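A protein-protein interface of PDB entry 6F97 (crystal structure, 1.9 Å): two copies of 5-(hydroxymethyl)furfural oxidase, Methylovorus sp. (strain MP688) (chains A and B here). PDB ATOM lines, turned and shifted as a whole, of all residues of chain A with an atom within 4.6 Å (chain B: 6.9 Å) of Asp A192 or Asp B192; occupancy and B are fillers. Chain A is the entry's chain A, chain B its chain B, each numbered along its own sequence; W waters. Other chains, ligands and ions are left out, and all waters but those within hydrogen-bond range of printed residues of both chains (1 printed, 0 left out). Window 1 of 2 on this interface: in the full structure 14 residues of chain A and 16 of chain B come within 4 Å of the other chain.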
ATOM      1  N   ILE A 184       5.328 -16.330 -28.598  1.00  0.00           N
ATOM      2  CA  ILE A 184       4.576 -16.349 -27.335  1.00  0.00           C
ATOM      3  C   ILE A 184       3.248 -15.586 -27.387  1.00  0.00           C
ATOM      4  O   ILE A 184       2.506 -15.604 -26.408  1.00  0.00           O
ATOM      5  CB  ILE A 184       5.418 -15.883 -26.157  1.00  0.00           C
ATOM      6  CG1 ILE A 184       5.717 -14.380 -26.220  1.00  0.00           C
ATOM      7  CG2 ILE A 184       6.694 -16.684 -26.108  1.00  0.00           C
ATOM      8  CD1 ILE A 184       6.130 -13.752 -24.888  1.00  0.00           C
ATOM      9  N   ARG A 190       2.124 -14.349 -20.603  1.00  0.00           N
ATOM     10  CA  ARG A 190       3.047 -15.433 -20.889  1.00  0.00           C
ATOM     11  C   ARG A 190       4.468 -14.894 -20.768  1.00  0.00           C
ATOM     12  O   ARG A 190       4.823 -13.887 -21.413  1.00  0.00           O
ATOM     13  CB  ARG A 190       2.831 -15.988 -22.292  1.00  0.00           C
ATOM     14  CG  ARG A 190       3.866 -17.053 -22.651  1.00  0.00           C
ATOM     15  CD  ARG A 190       3.537 -17.916 -23.873  1.00  0.00           C
ATOM     16  NE  ARG A 190       4.701 -18.805 -24.137  1.00  0.00           N
ATOM     17  CZ  ARG A 190       4.783 -19.725 -25.087  1.00  0.00           C
ATOM     18  NH1 ARG A 190       3.768 -19.947 -25.885  1.00  0.00           N
ATOM     19  NH2 ARG A 190       5.886 -20.427 -25.234  1.00  0.00           N
ATOM     20  N   PHE A 191       5.260 -15.566 -19.927  1.00  0.00           N
ATOM     21  CA  PHE A 191       6.464 -15.018 -19.306  1.00  0.00           C
ATOM     22  C   PHE A 191       7.733 -15.792 -19.633  1.00  0.00           C
ATOM     23  O   PHE A 191       8.768 -15.588 -18.957  1.00  0.00           O
ATOM     24  CB  PHE A 191       6.212 -14.911 -17.792  1.00  0.00           C
ATOM     25  CG  PHE A 191       4.948 -14.120 -17.471  1.00  0.00           C
ATOM     26  CD1 PHE A 191       4.770 -12.823 -17.975  1.00  0.00           C
ATOM     27  CD2 PHE A 191       3.921 -14.673 -16.736  1.00  0.00           C
ATOM     28  CE1 PHE A 191       3.615 -12.105 -17.742  1.00  0.00           C
ATOM     29  CE2 PHE A 191       2.753 -13.944 -16.495  1.00  0.00           C
ATOM     30  CZ  PHE A 191       2.604 -12.658 -16.982  1.00  0.00           C
ATOM     31  N   ASP A 192       7.697 -16.691 -20.638  1.00  0.00           N
ATOM     32  CA  ASP A 192       8.967 -17.339 -21.082  1.00  0.00           C
ATOM     33  C   ASP A 192       9.595 -16.591 -22.284  1.00  0.00           C
ATOM     34  O   ASP A 192       8.963 -15.712 -22.930  1.00  0.00           O
ATOM     35  CB  ASP A 192       8.847 -18.828 -21.395  1.00  0.00           C
ATOM     36  CG  ASP A 192       7.801 -19.143 -22.462  1.00  0.00           C
ATOM     37  OD1 ASP A 192       6.854 -18.332 -22.665  1.00  0.00           O
ATOM     38  OD2 ASP A 192       7.865 -20.237 -23.064  1.00  0.00           O
ATOM     39  N   ASP A 193      10.831 -16.964 -22.583  1.00  0.00           N
ATOM     40  CA  ASP A 193      11.534 -16.429 -23.766  1.00  0.00           C
ATOM     41  C   ASP A 193      10.838 -16.679 -25.072  1.00  0.00           C
ATOM     42  O   ASP A 193      10.186 -17.706 -25.272  1.00  0.00           O
ATOM     43  CB  ASP A 193      12.970 -16.944 -23.800  1.00  0.00           C
ATOM     44  CG  ASP A 193      13.814 -16.300 -22.762  1.00  0.00           C
ATOM     45  OD1 ASP A 193      13.410 -15.284 -22.167  1.00  0.00           O
ATOM     46  OD2 ASP A 193      14.929 -16.763 -22.524  1.00  0.00           O
ATOM     47  N   GLY A 194      10.981 -15.734 -25.992  1.00  0.00           N
ATOM     48  CA  GLY A 194      10.395 -15.901 -27.348  1.00  0.00           C
ATOM     49  C   GLY A 194      10.017 -14.558 -27.962  1.00  0.00           C
ATOM     50  O   GLY A 194      10.425 -13.513 -27.490  1.00  0.00           O
ATOM     51  N   ARG A 338      11.894 -11.404 -26.203  1.00  0.00           N
ATOM     52  CA  ARG A 338      12.401 -11.620 -24.877  1.00  0.00           C
ATOM     53  C   ARG A 338      13.407 -12.781 -24.927  1.00  0.00           C
ATOM     54  O   ARG A 338      13.065 -13.901 -25.393  1.00  0.00           O
ATOM     55  CB  ARG A 338      11.230 -11.958 -23.952  1.00  0.00           C
ATOM     56  CG  ARG A 338      11.618 -12.220 -22.509  1.00  0.00           C
ATOM     57  CD  ARG A 338      10.427 -12.817 -21.743  1.00  0.00           C
ATOM     58  NE  ARG A 338       9.336 -11.896 -21.627  1.00  0.00           N
ATOM     59  CZ  ARG A 338       8.039 -12.168 -21.649  1.00  0.00           C
ATOM     60  NH1 ARG A 338       7.590 -13.390 -21.871  1.00  0.00           N
ATOM     61  NH2 ARG A 338       7.157 -11.156 -21.458  1.00  0.00           N
ATOM     62  N   LEU B 110      13.243 -27.998 -19.584  1.00  0.00           N
ATOM     63  CA  LEU B 110      13.283 -26.583 -20.003  1.00  0.00           C
ATOM     64  C   LEU B 110      14.540 -26.328 -20.818  1.00  0.00           C
ATOM     65  O   LEU B 110      15.520 -27.011 -20.625  1.00  0.00           O
ATOM     66  CB  LEU B 110      13.267 -25.642 -18.790  1.00  0.00           C
ATOM     67  CG  LEU B 110      12.171 -25.895 -17.749  1.00  0.00           C
ATOM     68  CD1 LEU B 110      12.332 -24.972 -16.564  1.00  0.00           C
ATOM     69  CD2 LEU B 110      10.788 -25.739 -18.313  1.00  0.00           C
ATOM     70  N   PRO B 182      -0.789 -18.760 -14.826  1.00  0.00           N
ATOM     71  CA  PRO B 182      -1.593 -19.080 -15.992  1.00  0.00           C
ATOM     72  C   PRO B 182      -1.700 -20.563 -16.204  1.00  0.00           C
ATOM     73  O   PRO B 182      -0.879 -21.322 -15.696  1.00  0.00           O
ATOM     74  CB  PRO B 182      -0.773 -18.476 -17.143  1.00  0.00           C
ATOM     75  CG  PRO B 182       0.630 -18.565 -16.665  1.00  0.00           C
ATOM     76  CD  PRO B 182       0.587 -18.370 -15.183  1.00  0.00           C
ATOM     77  N   ILE B 184      -0.689 -22.906 -18.744  1.00  0.00           N
ATOM     78  CA  ILE B 184       0.282 -22.835 -19.830  1.00  0.00           C
ATOM     79  C   ILE B 184      -0.057 -23.792 -20.981  1.00  0.00           C
ATOM     80  O   ILE B 184       0.596 -23.740 -22.029  1.00  0.00           O
ATOM     81  CB  ILE B 184       1.729 -23.029 -19.350  1.00  0.00           C
ATOM     82  CG1 ILE B 184       1.979 -24.445 -18.777  1.00  0.00           C
ATOM     83  CG2 ILE B 184       2.073 -21.951 -18.320  1.00  0.00           C
ATOM     84  CD1 ILE B 184       3.442 -24.705 -18.493  1.00  0.00           C
ATOM     85  N   ALA B 189       6.081 -27.126 -24.915  1.00  0.00           N
ATOM     86  CA  ALA B 189       6.551 -26.022 -25.789  1.00  0.00           C
ATOM     87  C   ALA B 189       6.445 -24.632 -25.154  1.00  0.00           C
ATOM     88  O   ALA B 189       6.713 -23.592 -25.824  1.00  0.00           O
ATOM     89  CB  ALA B 189       5.794 -26.059 -27.101  1.00  0.00           C
ATOM     90  N   ARG B 190       6.078 -24.606 -23.880  1.00  0.00           N
ATOM     91  CA  ARG B 190       5.923 -23.361 -23.143  1.00  0.00           C
ATOM     92  C   ARG B 190       6.522 -23.580 -21.782  1.00  0.00           C
ATOM     93  O   ARG B 190       6.219 -24.572 -21.122  1.00  0.00           O
ATOM     94  CB  ARG B 190       4.462 -22.941 -23.044  1.00  0.00           C
ATOM     95  CG  ARG B 190       4.258 -21.702 -22.157  1.00  0.00           C
ATOM     96  CD  ARG B 190       2.884 -21.056 -22.290  1.00  0.00           C
ATOM     97  NE  ARG B 190       2.780 -20.049 -21.227  1.00  0.00           N
ATOM     98  CZ  ARG B 190       1.734 -19.281 -20.936  1.00  0.00           C
ATOM     99  NH1 ARG B 190       0.590 -19.404 -21.577  1.00  0.00           N
ATOM    100  NH2 ARG B 190       1.839 -18.447 -19.914  1.00  0.00           N
ATOM    101  N   PHE B 191       7.409 -22.660 -21.387  1.00  0.00           N
ATOM    102  CA  PHE B 191       8.397 -22.920 -20.362  1.00  0.00           C
ATOM    103  C   PHE B 191       8.365 -21.958 -19.194  1.00  0.00           C
ATOM    104  O   PHE B 191       9.299 -21.898 -18.468  1.00  0.00           O
ATOM    105  CB  PHE B 191       9.800 -22.974 -21.018  1.00  0.00           C
ATOM    106  CG  PHE B 191       9.892 -23.993 -22.150  1.00  0.00           C
ATOM    107  CD1 PHE B 191       9.604 -25.336 -21.911  1.00  0.00           C
ATOM    108  CD2 PHE B 191      10.207 -23.597 -23.470  1.00  0.00           C
ATOM    109  CE1 PHE B 191       9.681 -26.281 -22.937  1.00  0.00           C
ATOM    110  CE2 PHE B 191      10.289 -24.541 -24.511  1.00  0.00           C
ATOM    111  CZ  PHE B 191      10.008 -25.889 -24.245  1.00  0.00           C
ATOM    112  N   ASP B 192       7.297 -21.205 -19.000  1.00  0.00           N
ATOM    113  CA  ASP B 192       7.204 -20.386 -17.775  1.00  0.00           C
ATOM    114  C   ASP B 192       6.474 -21.190 -16.653  1.00  0.00           C
ATOM    115  O   ASP B 192       5.833 -22.210 -16.900  1.00  0.00           O
ATOM    116  CB  ASP B 192       6.575 -18.992 -18.073  1.00  0.00           C
ATOM    117  CG  ASP B 192       5.152 -19.046 -18.736  1.00  0.00           C
ATOM    118  OD1 ASP B 192       4.803 -20.028 -19.397  1.00  0.00           O
ATOM    119  OD2 ASP B 192       4.328 -18.096 -18.559  1.00  0.00           O
ATOM    120  N   ASP B 193       6.569 -20.711 -15.428  1.00  0.00           N
ATOM    121  CA  ASP B 193       5.688 -21.196 -14.358  1.00  0.00           C
ATOM    122  C   ASP B 193       4.166 -21.132 -14.699  1.00  0.00           C
ATOM    123  O   ASP B 193       3.692 -20.232 -15.368  1.00  0.00           O
ATOM    124  CB  ASP B 193       6.006 -20.417 -13.065  1.00  0.00           C
ATOM    125  CG  ASP B 193       7.353 -20.817 -12.461  1.00  0.00           C
ATOM    126  OD1 ASP B 193       7.944 -21.857 -12.886  1.00  0.00           O
ATOM    127  OD2 ASP B 193       7.804 -20.136 -11.533  1.00  0.00           O
ATOM    128  N   GLY B 194       3.428 -22.136 -14.247  1.00  0.00           N
ATOM    129  CA  GLY B 194       1.983 -22.232 -14.436  1.00  0.00           C
ATOM    130  C   GLY B 194       1.509 -23.665 -14.249  1.00  0.00           C
ATOM    131  O   GLY B 194       2.284 -24.550 -13.782  1.00  0.00           O
ATOM    132  N   TYR B 195       0.241 -23.890 -14.618  1.00  0.00           N
ATOM    133  CA  TYR B 195      -0.396 -25.161 -14.467  1.00  0.00           C
ATOM    134  C   TYR B 195      -0.876 -25.600 -15.826  1.00  0.00           C
ATOM    135  O   TYR B 195      -0.960 -24.797 -16.770  1.00  0.00           O
ATOM    136  CB  TYR B 195      -1.542 -25.107 -13.408  1.00  0.00           C
ATOM    137  CG  TYR B 195      -2.737 -24.241 -13.787  1.00  0.00           C
ATOM    138  CD1 TYR B 195      -2.828 -22.906 -13.328  1.00  0.00           C
ATOM    139  CD2 TYR B 195      -3.728 -24.716 -14.609  1.00  0.00           C
ATOM    140  CE1 TYR B 195      -3.902 -22.093 -13.650  1.00  0.00           C
ATOM    141  CE2 TYR B 195      -4.816 -23.874 -14.953  1.00  0.00           C
ATOM    142  CZ  TYR B 195      -4.870 -22.591 -14.459  1.00  0.00           C
ATOM    143  OH  TYR B 195      -5.862 -21.770 -14.802  1.00  0.00           O
ATOM    144  N   PHE B 196      -1.168 -26.891 -15.932  1.00  0.00           N
ATOM    145  CA  PHE B 196      -1.438 -27.509 -17.202  1.00  0.00           C
ATOM    146  C   PHE B 196      -1.993 -28.898 -17.033  1.00  0.00           C
ATOM    147  O   PHE B 196      -1.672 -29.563 -16.042  1.00  0.00           O
ATOM    148  CB  PHE B 196      -0.150 -27.626 -18.013  1.00  0.00           C
ATOM    149  CG  PHE B 196       1.024 -28.151 -17.222  1.00  0.00           C
ATOM    150  CD1 PHE B 196       1.846 -27.288 -16.520  1.00  0.00           C
ATOM    151  CD2 PHE B 196       1.289 -29.507 -17.146  1.00  0.00           C
ATOM    152  CE1 PHE B 196       2.929 -27.772 -15.780  1.00  0.00           C
ATOM    153  CE2 PHE B 196       2.354 -29.987 -16.391  1.00  0.00           C
ATOM    154  CZ  PHE B 196       3.178 -29.127 -15.711  1.00  0.00           C
ATOM    155  N   ARG B 338       4.161 -26.225 -12.500  1.00  0.00           N
ATOM    156  CA  ARG B 338       5.552 -25.845 -12.509  1.00  0.00           C
ATOM    157  C   ARG B 338       5.667 -24.595 -11.649  1.00  0.00           C
ATOM    158  O   ARG B 338       5.019 -23.585 -11.940  1.00  0.00           O
ATOM    159  CB  ARG B 338       5.971 -25.582 -13.975  1.00  0.00           C
ATOM    160  CG  ARG B 338       7.432 -25.218 -14.169  1.00  0.00           C
ATOM    161  CD  ARG B 338       7.722 -24.812 -15.563  1.00  0.00           C
ATOM    162  NE  ARG B 338       7.689 -25.902 -16.531  1.00  0.00           N
ATOM    163  CZ  ARG B 338       7.219 -25.834 -17.764  1.00  0.00           C
ATOM    164  NH1 ARG B 338       6.594 -24.732 -18.234  1.00  0.00           N
ATOM    165  NH2 ARG B 338       7.312 -26.903 -18.538  1.00  0.00           N
ATOM    166  N   ALA B 339       6.491 -24.605 -10.612  1.00  0.00           N
ATOM    167  CA  ALA B 339       6.621 -23.419  -9.760  1.00  0.00           C
ATOM    168  C   ALA B 339       8.047 -23.144  -9.373  1.00  0.00           C
ATOM    169  O   ALA B 339       8.904 -24.005  -9.521  1.00  0.00           O
ATOM    170  CB  ALA B 339       5.769 -23.556  -8.495  1.00  0.00           C
ATOM    171  N   SER B 349      11.746 -22.338 -11.636  1.00  0.00           N
ATOM    172  CA  SER B 349      11.020 -23.519 -12.063  1.00  0.00           C
ATOM    173  C   SER B 349      11.572 -24.847 -11.470  1.00  0.00           C
ATOM    174  O   SER B 349      11.603 -25.897 -12.123  1.00  0.00           O
ATOM    175  CB  SER B 349      10.962 -23.541 -13.600  1.00  0.00           C
ATOM    176  OG  SER B 349      10.190 -22.434 -14.050  1.00  0.00           O
HETATM  177  O   HOH W   1       4.948 -22.491 -27.357  1.00  0.00           O
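Water W1 bridges the backbone carbonyl oxygen of Ala B189 (2.6 Å) and the guanidinium group of Arg A190 (3.1 Å).
Arg A190 touches its own counterpart, Arg B190. Arg A190 touches Asp B192, and with the chains exchanged Asp A192 touches Arg B190. Phe A191 touches Asp B192, and with the chains exchanged Asp A192 touches Phe B191. Asp B192 touches its own counterpart, Asp A192. Of the 7 pairs that touch across the chains among the printed residues, 6 have their exchanged pair printed and touching as well.
NH2 of Arg A190 sits at hydrogen-bond distance from O of Ala B189 (3.3 Å). The backbone NH of Phe A191 lies within hydrogen-bond range of the side-chain carboxylate of Asp B192, 3.0 Å away. N of Phe B191 sits at hydrogen-bond distance from OD2 of Asp A192.
Among the printed residues, pairs that only touch across the chains: Arg A190 with Arg B190 (3.4 Å), Arg A190 with Asp B192 (3.8 Å), Asp A192 with Arg B190 (3.7 Å) and Asp A192 with Asp B192 (3.6 Å).
Of the 7 printed residues of chain A, 3 touch a printed residue of chain B. Hydrophobic or aromatic side chains of chain A within 4 Å of the printed part of chain B: Phe A191.
Asp A192 touches just these residues of chain B: Arg B190 (3.7 Å), Phe B191 (3.0 Å) and Asp B192 (3.6 Å). Of chain A, only Arg A190, Phe A191 and Asp A192 come within 4 Å of Asp B192. Of the printed residues of chain A, Phe B191 touches Asp A192. Of the printed residues of chain B, Phe A191 touches Asp B192 (3.0 Å). Printed residues of chain B within 4 Å of Arg A190: Ala B189 (3.3 Å), Arg B190 (3.4 Å) and Asp B192 (3.8 Å). Printed residues of chain A within 4 Å of Ala B189: Arg A190 (3.3 Å). Of the printed residues of chain A, Arg B190 touches Arg A190 and Asp A192. Ala B339 touches none of the printed residues of chain A. The nearest printed residue of chain A that does not touch Asp B192 is Asp A193 (6.5 Å). The nearest printed residue of chain B that does not touch Arg A190 is Phe B191 (4.7 Å).
NE of Arg A190 lies within salt-bridge range of OD1 of Asp A192. The backbone carbonyl oxygen of Arg A190 lies within hydrogen-bond range of the guanidinium group of Arg A338 (2.8 Å). The backbone carbonyl oxygen (O) of Asp A192 lies within hydrogen-bond range of the guanidinium group (NH1) of Arg A338 (2.9 Å). NE of Arg B190 lies within salt-bridge range of OD1 of Asp B192 (2.7 Å). The guanidinium group of Arg B338 is in hydrogen-bond range of the backbone carbonyl oxygen of Arg B190, at 2.9 Å. The backbone carbonyl oxygen (O) of Asp B192 lies within hydrogen-bond range of the guanidinium group (NH1) of Arg B338.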
